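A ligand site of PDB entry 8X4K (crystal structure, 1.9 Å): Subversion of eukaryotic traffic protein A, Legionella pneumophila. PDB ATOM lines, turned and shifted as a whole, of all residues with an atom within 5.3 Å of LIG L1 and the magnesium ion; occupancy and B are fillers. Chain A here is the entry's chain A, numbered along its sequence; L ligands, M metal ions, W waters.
O of Ile 11 is in hydrogen-bond range of O3 of LIG L1 (2.6 Å).
The backbone NH (N) of Ala 252 lies within hydrogen-bond range of an oxygen (O12) of LIG L1 (2.7 Å).
An oxygen (O3) of LIG L1 sits at hydrogen-bond distance from the side-chain hydroxyl (OG) of Ser 93 (2.7 Å).
N of Val 13 lies within hydrogen-bond range of O1 of LIG L1 (2.8 Å).
The backbone carbonyl oxygen of Val 13 sits at hydrogen-bond distance from a nitrogen (N2) of LIG L1 (2.9 Å).
An oxygen (O12) of LIG L1 is in hydrogen-bond range of the side-chain amide nitrogen (ND2) of Asn 250 (2.8 Å).
The indole nitrogen (NE1) of Trp 254 lies within hydrogen-bond range of an oxygen (O11) of LIG L1.
O8 of LIG L1 sits at hydrogen-bond distance from N of Ser 253, at 2.9 Å.
O8 of LIG L1 is in hydrogen-bond range of OG of Ser 253 (2.8 Å).
The backbone NH (N) of Asp 251 is in hydrogen-bond range of an oxygen (O12) of LIG L1 (3.4 Å).
OH of Tyr 108 lies within hydrogen-bond range of O5 of LIG L1.
An oxygen (O10) of LIG L1 sits close to the side-chain amide nitrogen of Gln 136 (3.5 Å).
The side-chain carboxylate of Asp 110 lies within hydrogen-bond range of an oxygen (O3) of LG2 L2 (3.0 Å).
The side-chain amide nitrogen (NE2) of Gln 136 sits at hydrogen-bond distance from an oxygen (O2) of LG2 L2.
The guanidinium group (NH2) of Arg 97 is in hydrogen-bond range of an oxygen (O3) of LG2 L2 (2.7 Å).
An oxygen (O2) of LG2 L2 lies close to the side-chain carboxylate (OD2) of Asp 145, 3.3 Å away.
An oxygen (O10) of LIG L1 lies close to an oxygen (O2) of LG2 L2, 2.9 Å away.
The side-chain carboxylate of Asp 112 sits close to the backbone NH of Asp 251, at 2.8 Å.
The side-chain carboxylate of Asp 110 sits at hydrogen-bond distance from the side-chain hydroxyl of Tyr 108 (2.6 Å).
NH1 of Arg 97 lies within salt-bridge range of OD1 of Asp 110 (3.6 Å).
The backbone carbonyl oxygen of Asp 145 is in hydrogen-bond range of the backbone NH of Asp 110 (3.2 Å).
The side-chain hydroxyl of Ser 93 sits at hydrogen-bond distance from the side-chain hydroxyl of Tyr 108, 3.4 Å away.
The side-chain hydroxyl of Ser 93 sits at hydrogen-bond distance from the guanidinium group of Arg 97 (2.8 Å).
NH1 of Arg 97 lies within hydrogen-bond range of OH of Tyr 108 (3.0 Å).
Trp 12 touches LIG L1.
CD2 of Tyr 89 touches O2 of LIG L1 (3.4 Å).
Hydrophobic or aromatic side chains that line LIG L1: Ile 11, Trp 12, Val 13, Tyr 89 and Trp 254.
Of the 19 residues printed, 14 come within 4 Å of LIG L1.
Of the 19 residues printed, 2 come within 4 Å of the magnesium ion.
The nearest printed residue that does not touch the magnesium ion is Asp 145 (4.4 Å).
The magnesium ion is bound by an oxygen (O10) of LIG L1, water W5, an oxygen (O7) of LIG L1, the side-chain carboxylate (OD1) of Asp 112, the side-chain carboxylate (OD2) of Asp 110 and the side-chain carboxylate (OD2) of Asp 112.
Water W5 bridges the side-chain carboxylate (OD2) of Asp 145 (2.6 Å) and an oxygen (O2) of LG2 L2 (3.5 Å).
Water W1 bridges O5 of LIG L1 (2.8 Å) and N of Ser 111 (3.0 Å).
Water W6 bridges an oxygen (O2) of LIG L1 and the backbone carbonyl oxygen (O) of Val 13.
Water W3 bridges OD2 of Asp 251 and O8 of LIG L1.
Water W2 lies within hydrogen-bond range of the backbone NH (N) of Ile 11 (2.8 Å), the side-chain hydroxyl (OH) of Tyr 108 (2.9 Å) and an oxygen (O5) of LIG L1 (3.3 Å).
Water W4 lies within hydrogen-bond range of the side-chain hydroxyl (OG) of Ser 111 (2.7 Å), the backbone carbonyl oxygen (O) of Ile 11 (2.8 Å) and an oxygen (O5) of LIG L1 (3.5 Å).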
ATOM      1  N   ILE A  11      27.533  -3.810   9.959  1.00  0.00           N
ATOM      2  CA  ILE A  11      26.981  -4.269  11.229  1.00  0.00           C
ATOM      3  C   ILE A  11      26.445  -5.701  11.062  1.00  0.00           C
ATOM      4  O   ILE A  11      25.634  -5.995  10.160  1.00  0.00           O
ATOM      5  CB  ILE A  11      25.863  -3.317  11.675  1.00  0.00           C
ATOM      6  CG1 ILE A  11      26.379  -1.918  11.958  1.00  0.00           C
ATOM      7  CG2 ILE A  11      25.045  -3.866  12.849  1.00  0.00           C
ATOM      8  CD1 ILE A  11      25.281  -0.924  12.094  1.00  0.00           C
ATOM      9  N   TRP A  12      26.756  -6.563  12.031  1.00  0.00           N
ATOM     10  CA  TRP A  12      26.013  -7.822  12.089  1.00  0.00           C
ATOM     11  C   TRP A  12      25.838  -8.253  13.543  1.00  0.00           C
ATOM     12  O   TRP A  12      26.815  -8.623  14.176  1.00  0.00           O
ATOM     13  CB  TRP A  12      26.655  -8.939  11.251  1.00  0.00           C
ATOM     14  CG  TRP A  12      25.650 -10.021  11.018  1.00  0.00           C
ATOM     15  CD1 TRP A  12      25.328 -11.055  11.859  1.00  0.00           C
ATOM     16  CD2 TRP A  12      24.732 -10.102   9.905  1.00  0.00           C
ATOM     17  NE1 TRP A  12      24.283 -11.773  11.342  1.00  0.00           N
ATOM     18  CE2 TRP A  12      23.879 -11.193  10.158  1.00  0.00           C
ATOM     19  CE3 TRP A  12      24.539  -9.349   8.753  1.00  0.00           C
ATOM     20  CZ2 TRP A  12      22.881 -11.579   9.268  1.00  0.00           C
ATOM     21  CZ3 TRP A  12      23.537  -9.702   7.897  1.00  0.00           C
ATOM     22  CH2 TRP A  12      22.718 -10.807   8.152  1.00  0.00           C
ATOM     23  N   VAL A  13      24.587  -8.229  14.020  1.00  0.00           N
ATOM     24  CA  VAL A  13      24.308  -8.612  15.402  1.00  0.00           C
ATOM     25  C   VAL A  13      23.459  -9.882  15.431  1.00  0.00           C
ATOM     26  O   VAL A  13      22.770 -10.197  14.459  1.00  0.00           O
ATOM     27  CB  VAL A  13      23.640  -7.475  16.166  1.00  0.00           C
ATOM     28  CG1 VAL A  13      24.629  -6.324  16.369  1.00  0.00           C
ATOM     29  CG2 VAL A  13      22.360  -6.987  15.490  1.00  0.00           C
ATOM     30  N   GLY A  14      23.475 -10.568  16.565  1.00  0.00           N
ATOM     31  CA  GLY A  14      22.745 -11.816  16.712  1.00  0.00           C
ATOM     32  C   GLY A  14      23.717 -12.987  16.663  1.00  0.00           C
ATOM     33  O   GLY A  14      24.634 -13.073  17.498  1.00  0.00           O
ATOM     34  N   TYR A  89      16.496  -7.136  14.208  1.00  0.00           N
ATOM     35  CA  TYR A  89      17.874  -6.737  13.944  1.00  0.00           C
ATOM     36  C   TYR A  89      17.934  -5.626  12.900  1.00  0.00           C
ATOM     37  O   TYR A  89      18.937  -4.931  12.772  1.00  0.00           O
ATOM     38  CB  TYR A  89      18.649  -7.959  13.473  1.00  0.00           C
ATOM     39  CG  TYR A  89      18.796  -9.067  14.480  1.00  0.00           C
ATOM     40  CD1 TYR A  89      19.308  -8.832  15.741  1.00  0.00           C
ATOM     41  CD2 TYR A  89      18.469 -10.377  14.148  1.00  0.00           C
ATOM     42  CE1 TYR A  89      19.518  -9.881  16.629  1.00  0.00           C
ATOM     43  CE2 TYR A  89      18.643 -11.420  15.032  1.00  0.00           C
ATOM     44  CZ  TYR A  89      19.200 -11.177  16.272  1.00  0.00           C
ATOM     45  OH  TYR A  89      19.260 -12.236  17.153  1.00  0.00           O
ATOM     46  N   GLY A  90      16.872  -5.475  12.087  1.00  0.00           N
ATOM     47  CA  GLY A  90      16.751  -4.328  11.216  1.00  0.00           C
ATOM     48  C   GLY A  90      16.631  -3.019  12.011  1.00  0.00           C
ATOM     49  O   GLY A  90      17.363  -2.070  11.768  1.00  0.00           O
ATOM     50  N   SER A  93      20.122  -2.464  13.748  1.00  0.00           N
ATOM     51  CA  SER A  93      21.122  -1.986  12.797  1.00  0.00           C
ATOM     52  C   SER A  93      20.811  -0.565  12.354  1.00  0.00           C
ATOM     53  O   SER A  93      21.754   0.232  12.216  1.00  0.00           O
ATOM     54  CB  SER A  93      21.238  -2.948  11.636  1.00  0.00           C
ATOM     55  OG  SER A  93      22.210  -2.520  10.697  1.00  0.00           O
ATOM     56  N   ARG A  97      23.759   2.135  13.180  1.00  0.00           N
ATOM     57  CA  ARG A  97      24.541   2.766  12.129  1.00  0.00           C
ATOM     58  C   ARG A  97      24.694   4.254  12.404  1.00  0.00           C
ATOM     59  O   ARG A  97      25.765   4.787  12.174  1.00  0.00           O
ATOM     60  CB  ARG A  97      24.011   2.496  10.706  1.00  0.00           C
ATOM     61  CG  ARG A  97      22.649   3.083  10.389  1.00  0.00           C
ATOM     62  CD  ARG A  97      22.043   2.433   9.154  1.00  0.00           C
ATOM     63  NE  ARG A  97      21.774   1.004   9.349  1.00  0.00           N
ATOM     64  CZ  ARG A  97      21.179   0.220   8.442  1.00  0.00           C
ATOM     65  NH1 ARG A  97      20.988  -1.066   8.695  1.00  0.00           N
ATOM     66  NH2 ARG A  97      20.784   0.750   7.298  1.00  0.00           N
ATOM     67  N   TYR A 108      28.765   3.986   6.280  1.00  0.00           N
ATOM     68  CA  TYR A 108      28.030   2.762   6.656  1.00  0.00           C
ATOM     69  C   TYR A 108      27.510   2.118   5.390  1.00  0.00           C
ATOM     70  O   TYR A 108      26.978   2.838   4.543  1.00  0.00           O
ATOM     71  CB  TYR A 108      26.815   3.025   7.541  1.00  0.00           C
ATOM     72  CG  TYR A 108      25.971   1.780   7.643  1.00  0.00           C
ATOM     73  CD1 TYR A 108      26.358   0.723   8.460  1.00  0.00           C
ATOM     74  CD2 TYR A 108      24.864   1.594   6.841  1.00  0.00           C
ATOM     75  CE1 TYR A 108      25.630  -0.445   8.523  1.00  0.00           C
ATOM     76  CE2 TYR A 108      24.118   0.430   6.892  1.00  0.00           C
ATOM     77  CZ  TYR A 108      24.505  -0.600   7.729  1.00  0.00           C
ATOM     78  OH  TYR A 108      23.778  -1.759   7.794  1.00  0.00           O
ATOM     79  N   ASP A 110      25.282  -1.558   3.980  1.00  0.00           N
ATOM     80  CA  ASP A 110      24.697  -2.889   4.237  1.00  0.00           C
ATOM     81  C   ASP A 110      25.630  -3.918   3.588  1.00  0.00           C
ATOM     82  O   ASP A 110      26.393  -3.516   2.703  1.00  0.00           O
ATOM     83  CB  ASP A 110      23.285  -3.046   3.671  1.00  0.00           C
ATOM     84  CG  ASP A 110      22.156  -2.462   4.496  1.00  0.00           C
ATOM     85  OD1 ASP A 110      22.429  -1.875   5.549  1.00  0.00           O
ATOM     86  OD2 ASP A 110      21.004  -2.617   4.062  1.00  0.00           O
ATOM     87  N   SER A 111      25.581  -5.180   4.028  1.00  0.00           N
ATOM     88  CA  SER A 111      26.409  -6.275   3.460  1.00  0.00           C
ATOM     89  C   SER A 111      25.705  -6.919   2.254  1.00  0.00           C
ATOM     90  O   SER A 111      26.171  -7.980   1.836  1.00  0.00           O
ATOM     91  CB  SER A 111      26.728  -7.279   4.559  1.00  0.00           C
ATOM     92  OG  SER A 111      25.582  -7.652   5.290  1.00  0.00           O
ATOM     93  N   ASP A 112      24.618  -6.326   1.751  1.00  0.00           N
ATOM     94  CA  ASP A 112      23.914  -6.789   0.561  1.00  0.00           C
ATOM     95  C   ASP A 112      24.020  -5.759  -0.565  1.00  0.00           C
ATOM     96  O   ASP A 112      23.120  -5.647  -1.390  1.00  0.00           O
ATOM     97  CB  ASP A 112      22.454  -7.124   0.862  1.00  0.00           C
ATOM     98  CG  ASP A 112      21.608  -5.988   1.392  1.00  0.00           C
ATOM     99  OD1 ASP A 112      22.172  -4.975   1.822  1.00  0.00           O
ATOM    100  OD2 ASP A 112      20.365  -6.122   1.347  1.00  0.00           O
ATOM    101  N   GLN A 136      19.426  -0.359  -3.699  1.00  0.00           N
ATOM    102  CA  GLN A 136      18.798  -1.613  -4.070  1.00  0.00           C
ATOM    103  C   GLN A 136      18.471  -1.604  -5.567  1.00  0.00           C
ATOM    104  O   GLN A 136      17.457  -2.124  -5.965  1.00  0.00           O
ATOM    105  CB  GLN A 136      17.523  -1.872  -3.264  1.00  0.00           C
ATOM    106  CG  GLN A 136      17.806  -1.907  -1.763  1.00  0.00           C
ATOM    107  CD  GLN A 136      16.601  -2.159  -0.887  1.00  0.00           C
ATOM    108  OE1 GLN A 136      15.465  -2.070  -1.319  1.00  0.00           O
ATOM    109  NE2 GLN A 136      16.840  -2.516   0.363  1.00  0.00           N
ATOM    110  N   ASP A 145      20.735   2.617   3.726  1.00  0.00           N
ATOM    111  CA  ASP A 145      21.682   1.506   3.649  1.00  0.00           C
ATOM    112  C   ASP A 145      23.048   1.990   3.183  1.00  0.00           C
ATOM    113  O   ASP A 145      24.005   1.217   3.159  1.00  0.00           O
ATOM    114  CB  ASP A 145      21.136   0.313   2.847  1.00  0.00           C
ATOM    115  CG  ASP A 145      20.694   0.629   1.424  1.00  0.00           C
ATOM    116  OD1 ASP A 145      20.699   1.850   1.053  1.00  0.00           O
ATOM    117  OD2 ASP A 145      20.292  -0.356   0.722  1.00  0.00           O
ATOM    118  N   ASN A 250      18.377  -6.939  -2.651  1.00  0.00           N
ATOM    119  CA  ASN A 250      18.575  -6.807  -1.210  1.00  0.00           C
ATOM    120  C   ASN A 250      18.252  -8.124  -0.539  1.00  0.00           C
ATOM    121  O   ASN A 250      17.612  -8.963  -1.160  1.00  0.00           O
ATOM    122  CB  ASN A 250      17.739  -5.680  -0.595  1.00  0.00           C
ATOM    123  CG  ASN A 250      16.256  -5.864  -0.842  1.00  0.00           C
ATOM    124  OD1 ASN A 250      15.817  -5.885  -1.989  1.00  0.00           O
ATOM    125  ND2 ASN A 250      15.484  -6.034   0.215  1.00  0.00           N
ATOM    126  N   ASP A 251      18.703  -8.326   0.725  1.00  0.00           N
ATOM    127  CA  ASP A 251      18.596  -9.631   1.358  1.00  0.00           C
ATOM    128  C   ASP A 251      17.343  -9.752   2.225  1.00  0.00           C
ATOM    129  O   ASP A 251      16.892 -10.861   2.429  1.00  0.00           O
ATOM    130  CB  ASP A 251      19.825  -9.977   2.215  1.00  0.00           C
ATOM    131  CG  ASP A 251      21.050 -10.377   1.438  1.00  0.00           C
ATOM    132  OD1 ASP A 251      20.876 -10.699   0.245  1.00  0.00           O
ATOM    133  OD2 ASP A 251      22.167 -10.317   2.003  1.00  0.00           O
ATOM    134  N   ALA A 252      16.785  -8.650   2.748  1.00  0.00           N
ATOM    135  CA  ALA A 252      15.701  -8.701   3.722  1.00  0.00           C
ATOM    136  C   ALA A 252      16.011  -9.683   4.866  1.00  0.00           C
ATOM    137  O   ALA A 252      15.132 -10.369   5.361  1.00  0.00           O
ATOM    138  CB  ALA A 252      14.396  -9.068   3.065  1.00  0.00           C
ATOM    139  N   SER A 253      17.256  -9.701   5.331  1.00  0.00           N
ATOM    140  CA  SER A 253      17.700 -10.720   6.280  1.00  0.00           C
ATOM    141  C   SER A 253      17.054 -10.551   7.656  1.00  0.00           C
ATOM    142  O   SER A 253      17.065 -11.475   8.461  1.00  0.00           O
ATOM    143  CB  SER A 253      19.193 -10.694   6.398  1.00  0.00           C
ATOM    144  OG  SER A 253      19.585  -9.468   6.987  1.00  0.00           O
ATOM    145  N   TRP A 254      16.590  -9.338   7.988  1.00  0.00           N
ATOM    146  CA  TRP A 254      15.983  -9.053   9.284  1.00  0.00           C
ATOM    147  C   TRP A 254      14.512  -9.434   9.369  1.00  0.00           C
ATOM    148  O   TRP A 254      13.912  -9.340  10.446  1.00  0.00           O
ATOM    149  CB  TRP A 254      16.136  -7.575   9.603  1.00  0.00           C
ATOM    150  CG  TRP A 254      15.598  -6.706   8.499  1.00  0.00           C
ATOM    151  CD1 TRP A 254      16.239  -6.328   7.358  1.00  0.00           C
ATOM    152  CD2 TRP A 254      14.278  -6.190   8.395  1.00  0.00           C
ATOM    153  NE1 TRP A 254      15.427  -5.556   6.576  1.00  0.00           N
ATOM    154  CE2 TRP A 254      14.211  -5.461   7.183  1.00  0.00           C
ATOM    155  CE3 TRP A 254      13.143  -6.252   9.207  1.00  0.00           C
ATOM    156  CZ2 TRP A 254      13.042  -4.813   6.760  1.00  0.00           C
ATOM    157  CZ3 TRP A 254      12.007  -5.602   8.802  1.00  0.00           C
ATOM    158  CH2 TRP A 254      11.960  -4.899   7.608  1.00  0.00           C
HETATM  159  N1  LIG L   1      21.014  -7.736  10.600  1.00  0.00           N
HETATM  160  C1  LIG L   1      21.699  -8.240  11.694  1.00  0.00           C
HETATM  161  N2  LIG L   1      21.448  -9.547  11.984  1.00  0.00           N
HETATM  162  C2  LIG L   1      20.572 -10.398  11.319  1.00  0.00           C
HETATM  163  C3  LIG L   1      19.892  -9.800  10.213  1.00  0.00           C
HETATM  164  C4  LIG L   1      20.132  -8.518   9.900  1.00  0.00           C
HETATM  165  O1  LIG L   1      22.486  -7.570  12.343  1.00  0.00           O
HETATM  166  O2  LIG L   1      20.454 -11.548  11.710  1.00  0.00           O
HETATM  167  C5  LIG L   1      21.250  -6.323  10.256  1.00  0.00           C
HETATM  168  C6  LIG L   1      22.561  -6.109   9.499  1.00  0.00           C
HETATM  169  O3  LIG L   1      23.197  -4.999  10.105  1.00  0.00           O
HETATM  170  C7  LIG L   1      22.085  -5.820   8.075  1.00  0.00           C
HETATM  171  C8  LIG L   1      20.760  -5.094   8.346  1.00  0.00           C
HETATM  172  O4  LIG L   1      20.194  -5.854   9.447  1.00  0.00           O
HETATM  173  O5  LIG L   1      22.996  -5.008   7.355  1.00  0.00           O
HETATM  174  C9  LIG L   1      19.792  -5.017   7.197  1.00  0.00           C
HETATM  175  O6  LIG L   1      19.652  -6.324   6.595  1.00  0.00           O
HETATM  176  P1  LIG L   1      19.460  -6.448   5.014  1.00  0.00           P
HETATM  177  O7  LIG L   1      20.457  -5.598   4.307  1.00  0.00           O
HETATM  178  O8  LIG L   1      19.378  -7.886   4.658  1.00  0.00           O
HETATM  179  O9  LIG L   1      18.022  -5.766   4.832  1.00  0.00           O
HETATM  180  P2  LIG L   1      17.358  -4.978   3.597  1.00  0.00           P
HETATM  181  O10 LIG L   1      18.392  -4.015   3.110  1.00  0.00           O
HETATM  182  O11 LIG L   1      16.171  -4.294   4.178  1.00  0.00           O
HETATM  183  O12 LIG L   1      16.994  -5.993   2.577  1.00  0.00           O
HETATM  184  C1  LG2 L   2      17.541  -0.829   4.420  1.00  0.00           C
HETATM  185  C2  LG2 L   2      18.210  -1.597   5.554  1.00  0.00           C
HETATM  186  C3  LG2 L   2      17.389  -1.468   6.835  1.00  0.00           C
HETATM  187  C4  LG2 L   2      15.996  -1.991   6.575  1.00  0.00           C
HETATM  188  C5  LG2 L   2      15.105  -1.910   7.787  1.00  0.00           C
HETATM  189  C6  LG2 L   2      16.061  -1.168   4.313  1.00  0.00           C
HETATM  190  O1  LG2 L   2      15.472  -0.243   3.459  1.00  0.00           O
HETATM  191  O2  LG2 L   2      18.175  -1.087   3.175  1.00  0.00           O
HETATM  192  O3  LG2 L   2      19.540  -1.137   5.760  1.00  0.00           O
HETATM  193  O4  LG2 L   2      17.978  -2.211   7.902  1.00  0.00           O
HETATM  194  O5  LG2 L   2      15.388  -1.157   5.578  1.00  0.00           O
HETATM  195  O6  LG2 L   2      14.769  -0.556   8.057  1.00  0.00           O
HETATM  196 MG    MG M   1      20.344  -4.251   2.687  1.00  0.00          MG
HETATM  197  O   HOH W   1      22.941  -6.281   4.899  1.00  0.00           O
HETATM  198  O   HOH W   2      26.028  -3.616   7.556  1.00  0.00           O
HETATM  199  O   HOH W   3      22.188  -8.937   4.413  1.00  0.00           O
HETATM  200  O   HOH W   4      26.241  -6.191   7.429  1.00  0.00           O
HETATM  201  O   HOH W   5      20.255  -2.943   1.091  1.00  0.00           O
HETATM  202  O   HOH W   6      21.759 -13.384  13.426  1.00  0.00           O
HETATM  203  O   HOH W   7      18.118 -13.238  11.729  1.00  0.00           O
HETATM  204  O   HOH W   8      13.629  -4.504   3.218  1.00  0.00           O
